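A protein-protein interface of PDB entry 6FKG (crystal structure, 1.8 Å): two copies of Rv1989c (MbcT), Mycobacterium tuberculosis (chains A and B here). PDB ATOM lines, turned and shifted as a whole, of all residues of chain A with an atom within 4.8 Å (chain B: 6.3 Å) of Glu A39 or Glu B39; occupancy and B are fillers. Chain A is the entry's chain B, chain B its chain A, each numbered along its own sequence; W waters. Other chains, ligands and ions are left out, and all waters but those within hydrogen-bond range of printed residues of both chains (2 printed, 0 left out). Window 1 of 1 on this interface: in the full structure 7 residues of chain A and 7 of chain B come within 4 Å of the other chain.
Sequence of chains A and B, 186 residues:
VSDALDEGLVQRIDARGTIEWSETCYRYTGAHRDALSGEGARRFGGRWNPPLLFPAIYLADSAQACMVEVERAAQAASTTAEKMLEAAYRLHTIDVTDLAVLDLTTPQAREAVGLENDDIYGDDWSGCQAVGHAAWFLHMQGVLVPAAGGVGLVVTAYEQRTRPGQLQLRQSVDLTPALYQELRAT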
ATOM      1  N   SER A  37      33.178 -20.972  19.010  1.00  0.00           N
ATOM      2  CA  SER A  37      31.743 -20.804  18.754  1.00  0.00           C
ATOM      3  C   SER A  37      31.056 -20.008  19.847  1.00  0.00           C
ATOM      4  O   SER A  37      31.346 -20.192  21.032  1.00  0.00           O
ATOM      5  CB  SER A  37      31.037 -22.157  18.615  1.00  0.00           C
ATOM      6  OG  SER A  37      29.626 -21.999  18.771  1.00  0.00           O
ATOM      7  N   GLY A  38      30.135 -19.121  19.458  1.00  0.00           N
ATOM      8  CA  GLY A  38      29.404 -18.334  20.442  1.00  0.00           C
ATOM      9  C   GLY A  38      27.895 -18.486  20.337  1.00  0.00           C
ATOM     10  O   GLY A  38      27.137 -17.664  20.851  1.00  0.00           O
ATOM     11  N   GLU A  39      27.457 -19.556  19.684  1.00  0.00           N
ATOM     12  CA  GLU A  39      26.038 -19.719  19.387  1.00  0.00           C
ATOM     13  C   GLU A  39      25.188 -20.059  20.620  1.00  0.00           C
ATOM     14  O   GLU A  39      24.003 -19.769  20.639  1.00  0.00           O
ATOM     15  CB  GLU A  39      25.849 -20.781  18.334  1.00  0.00           C
ATOM     16  CG  GLU A  39      26.587 -20.437  17.067  1.00  0.00           C
ATOM     17  CD  GLU A  39      26.055 -19.175  16.404  1.00  0.00           C
ATOM     18  OE1 GLU A  39      24.849 -18.870  16.569  1.00  0.00           O
ATOM     19  OE2 GLU A  39      26.858 -18.490  15.727  1.00  0.00           O
ATOM     20  N   GLY A  40      25.795 -20.674  21.627  1.00  0.00           N
ATOM     21  CA  GLY A  40      25.055 -21.062  22.815  1.00  0.00           C
ATOM     22  C   GLY A  40      24.591 -19.846  23.597  1.00  0.00           C
ATOM     23  O   GLY A  40      23.435 -19.770  24.054  1.00  0.00           O
ATOM     24  N   ALA A  41      25.500 -18.891  23.754  1.00  0.00           N
ATOM     25  CA  ALA A  41      25.175 -17.631  24.398  1.00  0.00           C
ATOM     26  C   ALA A  41      24.107 -16.890  23.601  1.00  0.00           C
ATOM     27  O   ALA A  41      23.252 -16.221  24.172  1.00  0.00           O
ATOM     28  CB  ALA A  41      26.427 -16.776  24.554  1.00  0.00           C
ATOM     29  N   ARG A  42      24.140 -17.012  22.278  1.00  0.00           N
ATOM     30  CA  ARG A  42      23.099 -16.386  21.468  1.00  0.00           C
ATOM     31  C   ARG A  42      21.742 -17.067  21.659  1.00  0.00           C
ATOM     32  O   ARG A  42      20.710 -16.405  21.723  1.00  0.00           O
ATOM     33  CB  ARG A  42      23.468 -16.411  19.982  1.00  0.00           C
ATOM     34  CG  ARG A  42      22.438 -15.750  19.095  1.00  0.00           C
ATOM     35  CD  ARG A  42      22.632 -16.145  17.643  1.00  0.00           C
ATOM     36  NE  ARG A  42      22.583 -14.982  16.778  1.00  0.00           N
ATOM     37  CZ  ARG A  42      23.189 -14.901  15.597  1.00  0.00           C
ATOM     38  NH1 ARG A  42      23.884 -15.935  15.127  1.00  0.00           N
ATOM     39  NH2 ARG A  42      23.097 -13.782  14.888  1.00  0.00           N
ATOM     40  N   ARG A  43      21.740 -18.394  21.729  1.00  0.00           N
ATOM     41  CA  ARG A  43      20.486 -19.116  21.827  1.00  0.00           C
ATOM     42  C   ARG A  43      19.798 -18.880  23.181  1.00  0.00           C
ATOM     43  O   ARG A  43      18.580 -18.688  23.228  1.00  0.00           O
ATOM     44  CB  ARG A  43      20.726 -20.612  21.585  1.00  0.00           C
ATOM     45  CG  ARG A  43      20.659 -20.981  20.102  1.00  0.00           C
ATOM     46  CD  ARG A  43      21.253 -22.347  19.798  1.00  0.00           C
ATOM     47  NE  ARG A  43      20.638 -23.416  20.579  1.00  0.00           N
ATOM     48  CZ  ARG A  43      19.554 -24.096  20.219  1.00  0.00           C
ATOM     49  NH1 ARG A  43      18.939 -23.822  19.073  1.00  0.00           N
ATOM     50  NH2 ARG A  43      19.093 -25.062  21.007  1.00  0.00           N
ATOM     51  N   PRO A  55      26.295 -13.783  18.508  1.00  0.00           N
ATOM     52  CA  PRO A  55      27.098 -14.775  19.218  1.00  0.00           C
ATOM     53  C   PRO A  55      27.969 -14.092  20.254  1.00  0.00           C
ATOM     54  O   PRO A  55      28.372 -12.933  20.083  1.00  0.00           O
ATOM     55  CB  PRO A  55      27.959 -15.420  18.116  1.00  0.00           C
ATOM     56  CG  PRO A  55      27.390 -14.955  16.816  1.00  0.00           C
ATOM     57  CD  PRO A  55      26.662 -13.673  17.084  1.00  0.00           C
ATOM     58  N   ARG B  27      32.175 -26.141  -0.033  1.00  0.00           N
ATOM     59  CA  ARG B  27      31.172 -25.294   0.572  1.00  0.00           C
ATOM     60  C   ARG B  27      31.577 -23.847   0.385  1.00  0.00           C
ATOM     61  O   ARG B  27      32.777 -23.541   0.415  1.00  0.00           O
ATOM     62  CB  ARG B  27      31.056 -25.616   2.062  1.00  0.00           C
ATOM     63  CG  ARG B  27      30.027 -24.798   2.745  1.00  0.00           C
ATOM     64  CD  ARG B  27      30.179 -24.870   4.231  1.00  0.00           C
ATOM     65  NE  ARG B  27      29.007 -24.265   4.826  1.00  0.00           N
ATOM     66  CZ  ARG B  27      28.805 -24.164   6.127  1.00  0.00           C
ATOM     67  NH1 ARG B  27      29.720 -24.625   6.984  1.00  0.00           N
ATOM     68  NH2 ARG B  27      27.692 -23.602   6.561  1.00  0.00           N
ATOM     69  N   ARG B  33      32.854 -16.486   8.174  1.00  0.00           N
ATOM     70  CA  ARG B  33      32.192 -17.633   8.801  1.00  0.00           C
ATOM     71  C   ARG B  33      33.089 -18.856   8.922  1.00  0.00           C
ATOM     72  O   ARG B  33      34.008 -19.057   8.128  1.00  0.00           O
ATOM     73  CB  ARG B  33      30.933 -18.007   8.024  1.00  0.00           C
ATOM     74  CG  ARG B  33      29.909 -16.901   7.962  1.00  0.00           C
ATOM     75  CD  ARG B  33      29.767 -16.203   9.311  1.00  0.00           C
ATOM     76  NE  ARG B  33      28.719 -15.191   9.264  1.00  0.00           N
ATOM     77  CZ  ARG B  33      27.441 -15.420   9.543  1.00  0.00           C
ATOM     78  NH1 ARG B  33      27.043 -16.627   9.934  1.00  0.00           N
ATOM     79  NH2 ARG B  33      26.562 -14.431   9.455  1.00  0.00           N
ATOM     80  N   SER B  37      30.616 -24.503  10.426  1.00  0.00           N
ATOM     81  CA  SER B  37      29.429 -24.094  11.175  1.00  0.00           C
ATOM     82  C   SER B  37      28.157 -24.501  10.447  1.00  0.00           C
ATOM     83  O   SER B  37      28.113 -24.516   9.214  1.00  0.00           O
ATOM     84  CB  SER B  37      29.415 -22.586  11.425  1.00  0.00           C
ATOM     85  OG  SER B  37      28.188 -22.199  12.027  1.00  0.00           O
ATOM     86  N   GLY B  38      27.122 -24.835  11.215  1.00  0.00           N
ATOM     87  CA  GLY B  38      25.841 -25.210  10.637  1.00  0.00           C
ATOM     88  C   GLY B  38      24.676 -24.479  11.272  1.00  0.00           C
ATOM     89  O   GLY B  38      23.525 -24.881  11.118  1.00  0.00           O
ATOM     90  N   GLU B  39      24.972 -23.407  11.996  1.00  0.00           N
ATOM     91  CA  GLU B  39      23.944 -22.695  12.747  1.00  0.00           C
ATOM     92  C   GLU B  39      22.981 -21.918  11.852  1.00  0.00           C
ATOM     93  O   GLU B  39      21.830 -21.693  12.231  1.00  0.00           O
ATOM     94  CB  GLU B  39      24.588 -21.748  13.750  1.00  0.00           C
ATOM     95  CG  GLU B  39      25.508 -22.474  14.683  1.00  0.00           C
ATOM     96  CD  GLU B  39      24.787 -23.510  15.514  1.00  0.00           C
ATOM     97  OE1 GLU B  39      23.594 -23.300  15.840  1.00  0.00           O
ATOM     98  OE2 GLU B  39      25.421 -24.545  15.815  1.00  0.00           O
ATOM     99  N   GLY B  40      23.463 -21.513  10.681  1.00  0.00           N
ATOM    100  CA  GLY B  40      22.642 -20.787   9.725  1.00  0.00           C
ATOM    101  C   GLY B  40      21.457 -21.624   9.282  1.00  0.00           C
ATOM    102  O   GLY B  40      20.304 -21.189   9.362  1.00  0.00           O
ATOM    103  N   ALA B  41      21.746 -22.842   8.845  1.00  0.00           N
ATOM    104  CA  ALA B  41      20.700 -23.770   8.452  1.00  0.00           C
ATOM    105  C   ALA B  41      19.773 -24.069   9.632  1.00  0.00           C
ATOM    106  O   ALA B  41      18.582 -24.287   9.444  1.00  0.00           O
ATOM    107  CB  ALA B  41      21.307 -25.051   7.900  1.00  0.00           C
ATOM    108  N   ARG B  42      20.304 -24.057  10.851  1.00  0.00           N
ATOM    109  CA  ARG B  42      19.460 -24.294  12.019  1.00  0.00           C
ATOM    110  C   ARG B  42      18.509 -23.122  12.257  1.00  0.00           C
ATOM    111  O   ARG B  42      17.341 -23.313  12.599  1.00  0.00           O
ATOM    112  CB  ARG B  42      20.298 -24.537  13.286  1.00  0.00           C
ATOM    113  CG  ARG B  42      19.443 -24.861  14.515  1.00  0.00           C
ATOM    114  CD  ARG B  42      20.243 -24.689  15.821  1.00  0.00           C
ATOM    115  NE  ARG B  42      19.951 -25.752  16.773  1.00  0.00           N
ATOM    116  CZ  ARG B  42      20.822 -26.227  17.662  1.00  0.00           C
ATOM    117  NH1 ARG B  42      22.051 -25.712  17.751  1.00  0.00           N
ATOM    118  NH2 ARG B  42      20.461 -27.217  18.470  1.00  0.00           N
ATOM    119  N   ARG B  43      19.018 -21.904  12.096  1.00  0.00           N
ATOM    120  CA  ARG B  43      18.225 -20.732  12.410  1.00  0.00           C
ATOM    121  C   ARG B  43      17.073 -20.566  11.409  1.00  0.00           C
ATOM    122  O   ARG B  43      15.955 -20.223  11.795  1.00  0.00           O
ATOM    123  CB  ARG B  43      19.112 -19.479  12.433  1.00  0.00           C
ATOM    124  CG  ARG B  43      20.017 -19.411  13.665  1.00  0.00           C
ATOM    125  CD  ARG B  43      20.904 -18.180  13.650  1.00  0.00           C
ATOM    126  NE  ARG B  43      20.123 -16.950  13.649  1.00  0.00           N
ATOM    127  CZ  ARG B  43      20.602 -15.767  13.287  1.00  0.00           C
ATOM    128  NH1 ARG B  43      21.860 -15.663  12.872  1.00  0.00           N
ATOM    129  NH2 ARG B  43      19.826 -14.694  13.325  1.00  0.00           N
ATOM    130  N   PHE B  44      17.354 -20.826  10.142  1.00  0.00           N
ATOM    131  CA  PHE B  44      16.395 -20.553   9.074  1.00  0.00           C
ATOM    132  C   PHE B  44      15.700 -21.794   8.538  1.00  0.00           C
ATOM    133  O   PHE B  44      14.575 -21.710   8.028  1.00  0.00           O
ATOM    134  CB  PHE B  44      17.082 -19.837   7.917  1.00  0.00           C
ATOM    135  CG  PHE B  44      16.124 -19.372   6.854  1.00  0.00           C
ATOM    136  CD1 PHE B  44      15.295 -18.287   7.090  1.00  0.00           C
ATOM    137  CD2 PHE B  44      16.053 -20.021   5.632  1.00  0.00           C
ATOM    138  CE1 PHE B  44      14.408 -17.845   6.115  1.00  0.00           C
ATOM    139  CE2 PHE B  44      15.165 -19.594   4.652  1.00  0.00           C
ATOM    140  CZ  PHE B  44      14.344 -18.500   4.899  1.00  0.00           C
ATOM    141  N   PHE B  54      18.614 -28.799  14.866  1.00  0.00           N
ATOM    142  CA  PHE B  54      20.022 -29.183  14.774  1.00  0.00           C
ATOM    143  C   PHE B  54      20.769 -28.393  13.715  1.00  0.00           C
ATOM    144  O   PHE B  54      20.175 -28.017  12.705  1.00  0.00           O
ATOM    145  CB  PHE B  54      20.155 -30.683  14.471  1.00  0.00           C
ATOM    146  CG  PHE B  54      19.327 -31.155  13.291  1.00  0.00           C
ATOM    147  CD1 PHE B  54      19.861 -31.169  12.008  1.00  0.00           C
ATOM    148  CD2 PHE B  54      18.029 -31.610  13.469  1.00  0.00           C
ATOM    149  CE1 PHE B  54      19.103 -31.603  10.930  1.00  0.00           C
ATOM    150  CE2 PHE B  54      17.271 -32.054  12.397  1.00  0.00           C
ATOM    151  CZ  PHE B  54      17.810 -32.053  11.122  1.00  0.00           C
ATOM    152  N   PRO B  55      22.077 -28.168  13.934  1.00  0.00           N
ATOM    153  CA  PRO B  55      22.919 -27.547  12.906  1.00  0.00           C
ATOM    154  C   PRO B  55      22.990 -28.449  11.696  1.00  0.00           C
ATOM    155  O   PRO B  55      22.895 -29.666  11.830  1.00  0.00           O
ATOM    156  CB  PRO B  55      24.294 -27.429  13.568  1.00  0.00           C
ATOM    157  CG  PRO B  55      24.035 -27.576  15.046  1.00  0.00           C
ATOM    158  CD  PRO B  55      22.828 -28.463  15.165  1.00  0.00           C
ATOM    159  N   ALA B  56      23.151 -27.860  10.521  1.00  0.00           N
ATOM    160  CA  ALA B  56      23.275 -28.642   9.315  1.00  0.00           C
ATOM    161  C   ALA B  56      24.202 -27.882   8.379  1.00  0.00           C
ATOM    162  O   ALA B  56      24.110 -26.657   8.278  1.00  0.00           O
ATOM    163  CB  ALA B  56      21.901 -28.879   8.669  1.00  0.00           C
ATOM    164  N   GLU B 159      29.085 -31.637  15.037  1.00  0.00           N
ATOM    165  CA  GLU B 159      29.880 -31.609  16.270  1.00  0.00           C
ATOM    166  C   GLU B 159      29.640 -32.824  17.165  1.00  0.00           C
ATOM    167  O   GLU B 159      30.592 -33.432  17.669  1.00  0.00           O
ATOM    168  CB  GLU B 159      29.592 -30.317  17.053  1.00  0.00           C
ATOM    169  CG  GLU B 159      29.759 -29.020  16.259  1.00  0.00           C
ATOM    170  CD  GLU B 159      28.604 -28.750  15.274  1.00  0.00           C
ATOM    171  OE1 GLU B 159      27.618 -29.526  15.257  1.00  0.00           O
ATOM    172  OE2 GLU B 159      28.689 -27.758  14.514  1.00  0.00           O
HETATM  173  O   HOH W   1      28.410 -22.949  16.217  1.00  0.00           O
HETATM  174  O   HOH W   2      28.595 -20.957  14.413  1.00  0.00           O
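Of chain B, only Glu B39 comes within 4 Å of Glu A39. Of chain A, only Glu A39 comes within 4 Å of Glu B39. Printed residues of chain B within 4 Å of Arg A43: Arg B42 (3.2 Å). Printed residues of chain A within 4 Å of Arg B43: Arg A42 (3.0 Å). Printed residues of chain A within 4 Å of Arg B42: Arg A43. The nearest residue of chain B that does not touch Glu A39 is Arg B43 (5.0 Å). The nearest residue of chain A that does not touch Glu B39 is Arg A43 (4.7 Å). The nearest printed residue of chain B that does not touch Arg A43 is Glu B39 (4.7 Å).
N of Glu B39 lies within hydrogen-bond range of OG of Ser B37 (3.4 Å). OE1 of Glu B39 lies within salt-bridge range of NH1 of Arg B42 (3.4 Å). OG of Ser A37 lies within hydrogen-bond range of N of Glu A39, 3.4 Å away. NH1 of Arg A42 lies within salt-bridge range of OE1 of Glu A39 (3.4 Å).
Printed residues of chain B that touch a printed residue of chain A: Glu B39, Arg B42 and Arg B43. Of the 8 printed residues of chain A, 3 touch a printed residue of chain B. Printed residues of chain A that touch a printed residue of chain B: Glu A39, Arg A42 and Arg A43. Among the printed residues, no Asp or Glu carboxylate lies within 4 Å of a Lys or Arg side-chain nitrogen of the other chain.
CG of Glu A39 touches CG of Glu B39 (3.3 Å).
The guanidinium group (NH2) of Arg A42 lies close to the guanidinium group (NH1) of Arg B43, at 3.0 Å. NH1 of Arg A43 sits close to NE of Arg B42 (3.2 Å).
Glu B39 touches its own counterpart, Glu A39. Arg A42 touches Arg B43, and with the chains exchanged Arg A43 touches Arg B42. Positions printed for both chains: 37, 38, 39, 40, 41, 42, 43 and 55. Of the 3 pairs that touch across the chains among the printed residues, 3 have their exchanged pair printed and touching as well.
Water W2 bridges the side-chain hydroxyl of Ser B37 (2.7 Å) and the side-chain carboxylate of Glu A39 (3.3 Å). Water W1 lies within hydrogen-bond range of OG of Ser A37 (3.0 Å) and OE2 of Glu B39 (3.4 Å).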
